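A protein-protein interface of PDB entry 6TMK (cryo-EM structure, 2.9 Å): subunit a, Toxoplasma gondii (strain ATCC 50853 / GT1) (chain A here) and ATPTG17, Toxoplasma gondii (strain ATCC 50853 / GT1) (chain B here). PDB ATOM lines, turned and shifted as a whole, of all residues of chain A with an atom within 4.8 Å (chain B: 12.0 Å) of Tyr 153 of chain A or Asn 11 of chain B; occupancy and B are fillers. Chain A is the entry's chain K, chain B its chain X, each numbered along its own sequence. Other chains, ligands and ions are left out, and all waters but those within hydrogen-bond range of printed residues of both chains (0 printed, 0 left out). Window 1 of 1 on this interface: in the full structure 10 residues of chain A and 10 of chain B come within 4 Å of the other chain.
Among the printed residues, merely in contact across the chains: Tyr 153 of chain A with Leu 15 of chain B, Tyr 156 of chain A with Pro 5 of chain B, Tyr 153 of chain A with Ala 8 of chain B, Phe 150 of chain A with Leu 12 of chain B, Met 157 of chain A with Phe 9 of chain B, Tyr 156 of chain A with Ala 8 of chain B and Tyr 153 of chain A with Asn 11 of chain B.
Tyr 153 of chain A touches just these residues of chain B: Ala 8 (3.5 Å), Asn 11 (3.96 Å) and Leu 15 (3.4 Å). Printed residues of chain A within 4 Å of Asn 11 of chain B: Tyr 153 (3.96 Å). Phe 150 of chain A touches one residue of chain B. No residue of chain B comes within 4 Å of Met 155 of chain A. Tyr 156 of chain A touches just these residues of chain B: Pro 5 (3.5 Å) and Ala 8 (3.9 Å). Of chain B, only Phe 9 comes within 4 Å of Met 157 of chain A. Of the printed residues of chain A, Pro 5 of chain B touches Tyr 156. Printed residues of chain A within 4 Å of Leu 12 of chain B: Phe 150. Printed residues of chain A within 4 Å of Leu 15 of chain B: Tyr 153. Printed residues of chain A within 4 Å of Phe 9 of chain B: Met 157. Leu 14 of chain B touches none of the printed residues of chain A. The nearest printed residue of chain A that does not touch Asn 11 of chain B is Phe 150 of chain A (6.6 Å). The nearest printed residue of chain A that does not touch Leu 15 of chain B is Phe 150 of chain A (4.4 Å).
Hydrophobic or aromatic side chains of chain B within 4 Å of the printed part of chain A: Pro 5, Ala 8, Phe 9, Leu 12 and Leu 15. Of the 9 printed residues of chain A, 4 touch a printed residue of chain B. Printed residues of chain A that touch a printed residue of chain B: Phe 150, Tyr 153, Tyr 156 and Met 157. Hydrophobic or aromatic side chains of chain A that line the printed part of chain B: Phe 150, Tyr 153, Tyr 156 and Met 157. Among the printed residues, 7 pairs touch across the chains. Among the printed residues, no Asp or Glu carboxylate lies within 4 Å of a Lys or Arg side-chain nitrogen of the other chain.
The backbone carbonyl oxygen (O) of Leu 7 of chain B sits at hydrogen-bond distance from the side-chain amide nitrogen (ND2) of Asn 11 of chain B. O of Phe 9 of chain B lies within hydrogen-bond range of OG1 of Thr 13 of chain B (2.7 Å).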
ATOM      1  N   ASN A 149      27.189 -14.361  13.297  1.00  0.00           N
ATOM      2  CA  ASN A 149      25.747 -14.169  13.186  1.00  0.00           C
ATOM      3  C   ASN A 149      25.093 -15.063  12.140  1.00  0.00           C
ATOM      4  O   ASN A 149      23.881 -14.949  11.941  1.00  0.00           O
ATOM      5  CB  ASN A 149      25.430 -12.712  12.851  1.00  0.00           C
ATOM      6  CG  ASN A 149      25.708 -11.769  13.999  1.00  0.00           C
ATOM      7  OD1 ASN A 149      26.363 -10.744  13.827  1.00  0.00           O
ATOM      8  ND2 ASN A 149      25.188 -12.094  15.170  1.00  0.00           N
ATOM      9  N   PHE A 150      25.840 -15.933  11.464  1.00  0.00           N
ATOM     10  CA  PHE A 150      25.241 -16.829  10.482  1.00  0.00           C
ATOM     11  C   PHE A 150      24.485 -17.987  11.117  1.00  0.00           C
ATOM     12  O   PHE A 150      23.797 -18.722  10.402  1.00  0.00           O
ATOM     13  CB  PHE A 150      26.310 -17.374   9.537  1.00  0.00           C
ATOM     14  CG  PHE A 150      26.519 -16.534   8.320  1.00  0.00           C
ATOM     15  CD1 PHE A 150      26.980 -15.240   8.428  1.00  0.00           C
ATOM     16  CD2 PHE A 150      26.244 -17.036   7.064  1.00  0.00           C
ATOM     17  CE1 PHE A 150      27.168 -14.466   7.310  1.00  0.00           C
ATOM     18  CE2 PHE A 150      26.429 -16.263   5.943  1.00  0.00           C
ATOM     19  CZ  PHE A 150      26.892 -14.976   6.067  1.00  0.00           C
ATOM     20  N   ARG A 151      24.597 -18.167  12.432  1.00  0.00           N
ATOM     21  CA  ARG A 151      23.878 -19.237  13.111  1.00  0.00           C
ATOM     22  C   ARG A 151      22.372 -19.017  13.091  1.00  0.00           C
ATOM     23  O   ARG A 151      21.598 -19.984  13.168  1.00  0.00           O
ATOM     24  CB  ARG A 151      24.387 -19.346  14.543  1.00  0.00           C
ATOM     25  CG  ARG A 151      24.123 -18.119  15.378  1.00  0.00           C
ATOM     26  CD  ARG A 151      24.844 -18.189  16.697  1.00  0.00           C
ATOM     27  NE  ARG A 151      24.540 -17.053  17.559  1.00  0.00           N
ATOM     28  CZ  ARG A 151      25.114 -15.860  17.455  1.00  0.00           C
ATOM     29  NH1 ARG A 151      24.778 -14.890  18.285  1.00  0.00           N
ATOM     30  NH2 ARG A 151      26.024 -15.635  16.522  1.00  0.00           N
ATOM     31  N   PHE A 152      21.938 -17.760  13.012  1.00  0.00           N
ATOM     32  CA  PHE A 152      20.513 -17.471  13.060  1.00  0.00           C
ATOM     33  C   PHE A 152      19.802 -18.028  11.838  1.00  0.00           C
ATOM     34  O   PHE A 152      18.662 -18.494  11.934  1.00  0.00           O
ATOM     35  CB  PHE A 152      20.295 -15.969  13.169  1.00  0.00           C
ATOM     36  CG  PHE A 152      20.708 -15.395  14.485  1.00  0.00           C
ATOM     37  CD1 PHE A 152      21.881 -14.681  14.604  1.00  0.00           C
ATOM     38  CD2 PHE A 152      19.925 -15.573  15.604  1.00  0.00           C
ATOM     39  CE1 PHE A 152      22.262 -14.156  15.809  1.00  0.00           C
ATOM     40  CE2 PHE A 152      20.303 -15.049  16.813  1.00  0.00           C
ATOM     41  CZ  PHE A 152      21.473 -14.339  16.917  1.00  0.00           C
ATOM     42  N   TYR A 153      20.464 -18.006  10.681  1.00  0.00           N
ATOM     43  CA  TYR A 153      19.862 -18.580   9.485  1.00  0.00           C
ATOM     44  C   TYR A 153      19.630 -20.072   9.656  1.00  0.00           C
ATOM     45  O   TYR A 153      18.578 -20.597   9.275  1.00  0.00           O
ATOM     46  CB  TYR A 153      20.766 -18.326   8.280  1.00  0.00           C
ATOM     47  CG  TYR A 153      21.093 -16.878   8.030  1.00  0.00           C
ATOM     48  CD1 TYR A 153      20.113 -15.973   7.666  1.00  0.00           C
ATOM     49  CD2 TYR A 153      22.389 -16.419   8.156  1.00  0.00           C
ATOM     50  CE1 TYR A 153      20.420 -14.654   7.434  1.00  0.00           C
ATOM     51  CE2 TYR A 153      22.702 -15.106   7.929  1.00  0.00           C
ATOM     52  CZ  TYR A 153      21.718 -14.225   7.571  1.00  0.00           C
ATOM     53  OH  TYR A 153      22.045 -12.910   7.345  1.00  0.00           O
ATOM     54  N   PHE A 154      20.609 -20.772  10.228  1.00  0.00           N
ATOM     55  CA  PHE A 154      20.473 -22.205  10.447  1.00  0.00           C
ATOM     56  C   PHE A 154      19.341 -22.503  11.422  1.00  0.00           C
ATOM     57  O   PHE A 154      18.519 -23.398  11.184  1.00  0.00           O
ATOM     58  CB  PHE A 154      21.802 -22.775  10.929  1.00  0.00           C
ATOM     59  CG  PHE A 154      22.876 -22.705   9.891  1.00  0.00           C
ATOM     60  CD1 PHE A 154      22.879 -23.574   8.818  1.00  0.00           C
ATOM     61  CD2 PHE A 154      23.875 -21.758   9.977  1.00  0.00           C
ATOM     62  CE1 PHE A 154      23.858 -23.501   7.858  1.00  0.00           C
ATOM     63  CE2 PHE A 154      24.858 -21.683   9.019  1.00  0.00           C
ATOM     64  CZ  PHE A 154      24.850 -22.555   7.960  1.00  0.00           C
ATOM     65  N   MET A 155      19.277 -21.747  12.518  1.00  0.00           N
ATOM     66  CA  MET A 155      18.182 -21.912  13.471  1.00  0.00           C
ATOM     67  C   MET A 155      16.834 -21.709  12.790  1.00  0.00           C
ATOM     68  O   MET A 155      15.901 -22.508  12.967  1.00  0.00           O
ATOM     69  CB  MET A 155      18.344 -20.928  14.625  1.00  0.00           C
ATOM     70  CG  MET A 155      19.545 -21.190  15.503  1.00  0.00           C
ATOM     71  SD  MET A 155      19.966 -19.784  16.547  1.00  0.00           S
ATOM     72  CE  MET A 155      21.387 -20.434  17.418  1.00  0.00           C
ATOM     73  N   TYR A 156      16.715 -20.638  12.006  1.00  0.00           N
ATOM     74  CA  TYR A 156      15.441 -20.314  11.380  1.00  0.00           C
ATOM     75  C   TYR A 156      15.029 -21.385  10.384  1.00  0.00           C
ATOM     76  O   TYR A 156      13.856 -21.772  10.335  1.00  0.00           O
ATOM     77  CB  TYR A 156      15.524 -18.961  10.681  1.00  0.00           C
ATOM     78  CG  TYR A 156      15.742 -17.782  11.595  1.00  0.00           C
ATOM     79  CD1 TYR A 156      15.269 -17.784  12.895  1.00  0.00           C
ATOM     80  CD2 TYR A 156      16.405 -16.653  11.146  1.00  0.00           C
ATOM     81  CE1 TYR A 156      15.467 -16.708  13.723  1.00  0.00           C
ATOM     82  CE2 TYR A 156      16.606 -15.573  11.965  1.00  0.00           C
ATOM     83  CZ  TYR A 156      16.133 -15.603  13.254  1.00  0.00           C
ATOM     84  OH  TYR A 156      16.334 -14.522  14.078  1.00  0.00           O
ATOM     85  N   MET A 157      15.970 -21.875   9.577  1.00  0.00           N
ATOM     86  CA  MET A 157      15.608 -22.900   8.607  1.00  0.00           C
ATOM     87  C   MET A 157      15.230 -24.201   9.299  1.00  0.00           C
ATOM     88  O   MET A 157      14.318 -24.904   8.849  1.00  0.00           O
ATOM     89  CB  MET A 157      16.756 -23.126   7.629  1.00  0.00           C
ATOM     90  CG  MET A 157      18.005 -23.665   8.264  1.00  0.00           C
ATOM     91  SD  MET A 157      19.276 -24.087   7.059  1.00  0.00           S
ATOM     92  CE  MET A 157      19.466 -22.523   6.217  1.00  0.00           C
ATOM     93  N   SER B   2      10.613  -6.869   4.461  1.00  0.00           N
ATOM     94  CA  SER B   2      12.062  -6.903   4.597  1.00  0.00           C
ATOM     95  C   SER B   2      12.572  -8.335   4.595  1.00  0.00           C
ATOM     96  O   SER B   2      13.010  -8.846   3.568  1.00  0.00           O
ATOM     97  CB  SER B   2      12.495  -6.198   5.882  1.00  0.00           C
ATOM     98  OG  SER B   2      12.231  -4.813   5.829  1.00  0.00           O
ATOM     99  N   THR B   3      12.504  -8.983   5.755  1.00  0.00           N
ATOM    100  CA  THR B   3      13.015 -10.332   5.926  1.00  0.00           C
ATOM    101  C   THR B   3      12.119 -11.086   6.897  1.00  0.00           C
ATOM    102  O   THR B   3      11.131 -10.555   7.410  1.00  0.00           O
ATOM    103  CB  THR B   3      14.455 -10.320   6.436  1.00  0.00           C
ATOM    104  OG1 THR B   3      14.538  -9.502   7.609  1.00  0.00           O
ATOM    105  CG2 THR B   3      15.380  -9.784   5.375  1.00  0.00           C
ATOM    106  N   SER B   4      12.481 -12.336   7.150  1.00  0.00           N
ATOM    107  CA  SER B   4      11.749 -13.191   8.068  1.00  0.00           C
ATOM    108  C   SER B   4      12.505 -14.495   8.267  1.00  0.00           C
ATOM    109  O   SER B   4      13.453 -14.786   7.527  1.00  0.00           O
ATOM    110  CB  SER B   4      10.345 -13.474   7.541  1.00  0.00           C
ATOM    111  OG  SER B   4      10.387 -13.913   6.195  1.00  0.00           O
ATOM    112  N   PRO B   5      12.129 -15.297   9.261  1.00  0.00           N
ATOM    113  CA  PRO B   5      12.794 -16.594   9.435  1.00  0.00           C
ATOM    114  C   PRO B   5      12.567 -17.540   8.276  1.00  0.00           C
ATOM    115  O   PRO B   5      13.449 -18.350   7.964  1.00  0.00           O
ATOM    116  CB  PRO B   5      12.170 -17.129  10.730  1.00  0.00           C
ATOM    117  CG  PRO B   5      11.690 -15.929  11.438  1.00  0.00           C
ATOM    118  CD  PRO B   5      11.238 -14.988  10.386  1.00  0.00           C
ATOM    119  N   GLY B   6      11.407 -17.465   7.627  1.00  0.00           N
ATOM    120  CA  GLY B   6      11.127 -18.321   6.494  1.00  0.00           C
ATOM    121  C   GLY B   6      11.984 -18.048   5.282  1.00  0.00           C
ATOM    122  O   GLY B   6      12.059 -18.897   4.388  1.00  0.00           O
ATOM    123  N   LEU B   7      12.628 -16.886   5.226  1.00  0.00           N
ATOM    124  CA  LEU B   7      13.487 -16.522   4.113  1.00  0.00           C
ATOM    125  C   LEU B   7      14.958 -16.766   4.400  1.00  0.00           C
ATOM    126  O   LEU B   7      15.815 -16.189   3.724  1.00  0.00           O
ATOM    127  CB  LEU B   7      13.279 -15.053   3.765  1.00  0.00           C
ATOM    128  CG  LEU B   7      11.864 -14.628   3.406  1.00  0.00           C
ATOM    129  CD1 LEU B   7      11.772 -13.123   3.371  1.00  0.00           C
ATOM    130  CD2 LEU B   7      11.472 -15.229   2.085  1.00  0.00           C
ATOM    131  N   ALA B   8      15.272 -17.602   5.387  1.00  0.00           N
ATOM    132  CA  ALA B   8      16.667 -17.859   5.706  1.00  0.00           C
ATOM    133  C   ALA B   8      17.374 -18.565   4.559  1.00  0.00           C
ATOM    134  O   ALA B   8      18.538 -18.274   4.264  1.00  0.00           O
ATOM    135  CB  ALA B   8      16.759 -18.681   6.986  1.00  0.00           C
ATOM    136  N   PHE B   9      16.679 -19.487   3.892  1.00  0.00           N
ATOM    137  CA  PHE B   9      17.244 -20.158   2.728  1.00  0.00           C
ATOM    138  C   PHE B   9      17.693 -19.148   1.683  1.00  0.00           C
ATOM    139  O   PHE B   9      18.851 -19.149   1.245  1.00  0.00           O
ATOM    140  CB  PHE B   9      16.213 -21.113   2.130  1.00  0.00           C
ATOM    141  CG  PHE B   9      15.726 -22.160   3.080  1.00  0.00           C
ATOM    142  CD1 PHE B   9      16.408 -23.351   3.229  1.00  0.00           C
ATOM    143  CD2 PHE B   9      14.569 -21.966   3.805  1.00  0.00           C
ATOM    144  CE1 PHE B   9      15.953 -24.316   4.095  1.00  0.00           C
ATOM    145  CE2 PHE B   9      14.110 -22.931   4.670  1.00  0.00           C
ATOM    146  CZ  PHE B   9      14.801 -24.106   4.814  1.00  0.00           C
ATOM    147  N   ALA B  10      16.774 -18.278   1.266  1.00  0.00           N
ATOM    148  CA  ALA B  10      17.081 -17.316   0.217  1.00  0.00           C
ATOM    149  C   ALA B  10      18.133 -16.317   0.673  1.00  0.00           C
ATOM    150  O   ALA B  10      19.009 -15.937  -0.109  1.00  0.00           O
ATOM    151  CB  ALA B  10      15.806 -16.599  -0.213  1.00  0.00           C
ATOM    152  N   ASN B  11      18.069 -15.879   1.929  1.00  0.00           N
ATOM    153  CA  ASN B  11      19.057 -14.939   2.444  1.00  0.00           C
ATOM    154  C   ASN B  11      20.457 -15.532   2.392  1.00  0.00           C
ATOM    155  O   ASN B  11      21.399 -14.895   1.907  1.00  0.00           O
ATOM    156  CB  ASN B  11      18.701 -14.531   3.869  1.00  0.00           C
ATOM    157  CG  ASN B  11      17.479 -13.652   3.935  1.00  0.00           C
ATOM    158  OD1 ASN B  11      17.170 -12.929   2.994  1.00  0.00           O
ATOM    159  ND2 ASN B  11      16.781 -13.703   5.052  1.00  0.00           N
ATOM    160  N   LEU B  12      20.611 -16.753   2.903  1.00  0.00           N
ATOM    161  CA  LEU B  12      21.910 -17.413   2.882  1.00  0.00           C
ATOM    162  C   LEU B  12      22.396 -17.603   1.454  1.00  0.00           C
ATOM    163  O   LEU B  12      23.551 -17.298   1.129  1.00  0.00           O
ATOM    164  CB  LEU B  12      21.803 -18.757   3.596  1.00  0.00           C
ATOM    165  CG  LEU B  12      23.096 -19.440   4.018  1.00  0.00           C
ATOM    166  CD1 LEU B  12      23.784 -18.647   5.103  1.00  0.00           C
ATOM    167  CD2 LEU B  12      22.784 -20.834   4.489  1.00  0.00           C
ATOM    168  N   THR B  13      21.519 -18.101   0.582  1.00  0.00           N
ATOM    169  CA  THR B  13      21.909 -18.351  -0.798  1.00  0.00           C
ATOM    170  C   THR B  13      22.377 -17.070  -1.470  1.00  0.00           C
ATOM    171  O   THR B  13      23.422 -17.047  -2.128  1.00  0.00           O
ATOM    172  CB  THR B  13      20.735 -18.956  -1.562  1.00  0.00           C
ATOM    173  OG1 THR B  13      20.225 -20.086  -0.848  1.00  0.00           O
ATOM    174  CG2 THR B  13      21.163 -19.384  -2.938  1.00  0.00           C
ATOM    175  N   LEU B  14      21.614 -15.991  -1.315  1.00  0.00           N
ATOM    176  CA  LEU B  14      21.995 -14.717  -1.908  1.00  0.00           C
ATOM    177  C   LEU B  14      23.331 -14.239  -1.363  1.00  0.00           C
ATOM    178  O   LEU B  14      24.267 -13.971  -2.126  1.00  0.00           O
ATOM    179  CB  LEU B  14      20.906 -13.685  -1.638  1.00  0.00           C
ATOM    180  CG  LEU B  14      19.608 -13.904  -2.408  1.00  0.00           C
ATOM    181  CD1 LEU B  14      18.503 -13.081  -1.805  1.00  0.00           C
ATOM    182  CD2 LEU B  14      19.778 -13.564  -3.877  1.00  0.00           C
ATOM    183  N   LEU B  15      23.439 -14.141  -0.036  1.00  0.00           N
ATOM    184  CA  LEU B  15      24.649 -13.615   0.577  1.00  0.00           C
ATOM    185  C   LEU B  15      25.879 -14.388   0.134  1.00  0.00           C
ATOM    186  O   LEU B  15      26.959 -13.806  -0.028  1.00  0.00           O
ATOM    187  CB  LEU B  15      24.521 -13.667   2.096  1.00  0.00           C
ATOM    188  CG  LEU B  15      23.568 -12.675   2.751  1.00  0.00           C
ATOM    189  CD1 LEU B  15      23.485 -12.965   4.226  1.00  0.00           C
ATOM    190  CD2 LEU B  15      24.004 -11.252   2.515  1.00  0.00           C
ATOM    191  N   LEU B  16      25.745 -15.696  -0.058  1.00  0.00           N
ATOM    192  CA  LEU B  16      26.896 -16.514  -0.403  1.00  0.00           C
ATOM    193  C   LEU B  16      27.151 -16.617  -1.899  1.00  0.00           C
ATOM    194  O   LEU B  16      28.276 -16.939  -2.292  1.00  0.00           O
ATOM    195  CB  LEU B  16      26.730 -17.919   0.179  1.00  0.00           C
ATOM    196  CG  LEU B  16      26.747 -17.999   1.710  1.00  0.00           C
ATOM    197  CD1 LEU B  16      26.541 -19.421   2.178  1.00  0.00           C
ATOM    198  CD2 LEU B  16      28.026 -17.438   2.285  1.00  0.00           C
ATOM    199  N   ASP B  17      26.156 -16.345  -2.741  1.00  0.00           N
ATOM    200  CA  ASP B  17      26.280 -16.571  -4.174  1.00  0.00           C
ATOM    201  C   ASP B  17      26.395 -15.310  -5.014  1.00  0.00           C
ATOM    202  O   ASP B  17      27.117 -15.319  -6.012  1.00  0.00           O
ATOM    203  CB  ASP B  17      25.078 -17.377  -4.670  1.00  0.00           C
ATOM    204  CG  ASP B  17      25.059 -18.793  -4.130  1.00  0.00           C
ATOM    205  OD1 ASP B  17      24.102 -19.532  -4.435  1.00  0.00           O
ATOM    206  OD2 ASP B  17      25.998 -19.166  -3.399  1.00  0.00           O
ATOM    207  N   VAL B  18      25.719 -14.219  -4.669  1.00  0.00           N
ATOM    208  CA  VAL B  18      25.820 -13.018  -5.499  1.00  0.00           C
ATOM    209  C   VAL B  18      27.216 -12.404  -5.446  1.00  0.00           C
ATOM    210  O   VAL B  18      27.612 -11.738  -6.413  1.00  0.00           O
ATOM    211  CB  VAL B  18      24.746 -11.976  -5.134  1.00  0.00           C
ATOM    212  CG1 VAL B  18      23.390 -12.626  -5.077  1.00  0.00           C
ATOM    213  CG2 VAL B  18      25.041 -11.285  -3.821  1.00  0.00           C
ATOM    214  N   PRO B  19      28.001 -12.574  -4.378  1.00  0.00           N
ATOM    215  CA  PRO B  19      29.405 -12.145  -4.453  1.00  0.00           C
ATOM    216  C   PRO B  19      30.252 -13.000  -5.373  1.00  0.00           C
ATOM    217  O   PRO B  19      31.310 -12.540  -5.820  1.00  0.00           O
ATOM    218  CB  PRO B  19      29.882 -12.259  -3.002  1.00  0.00           C
ATOM    219  CG  PRO B  19      28.647 -12.237  -2.200  1.00  0.00           C
ATOM    220  CD  PRO B  19      27.679 -13.006  -3.011  1.00  0.00           C
ATOM    221  N   GLN B  20      29.830 -14.227  -5.663  1.00  0.00           N
ATOM    222  CA  GLN B  20      30.581 -15.127  -6.524  1.00  0.00           C
ATOM    223  C   GLN B  20      30.381 -14.849  -8.005  1.00  0.00           C
ATOM    224  O   GLN B  20      31.142 -15.374  -8.822  1.00  0.00           O
ATOM    225  CB  GLN B  20      30.188 -16.568  -6.225  1.00  0.00           C
ATOM    226  CG  GLN B  20      30.467 -16.981  -4.811  1.00  0.00           C
ATOM    227  CD  GLN B  20      30.266 -18.453  -4.586  1.00  0.00           C
ATOM    228  OE1 GLN B  20      29.832 -19.178  -5.479  1.00  0.00           O
ATOM    229  NE2 GLN B  20      30.585 -18.910  -3.389  1.00  0.00           N
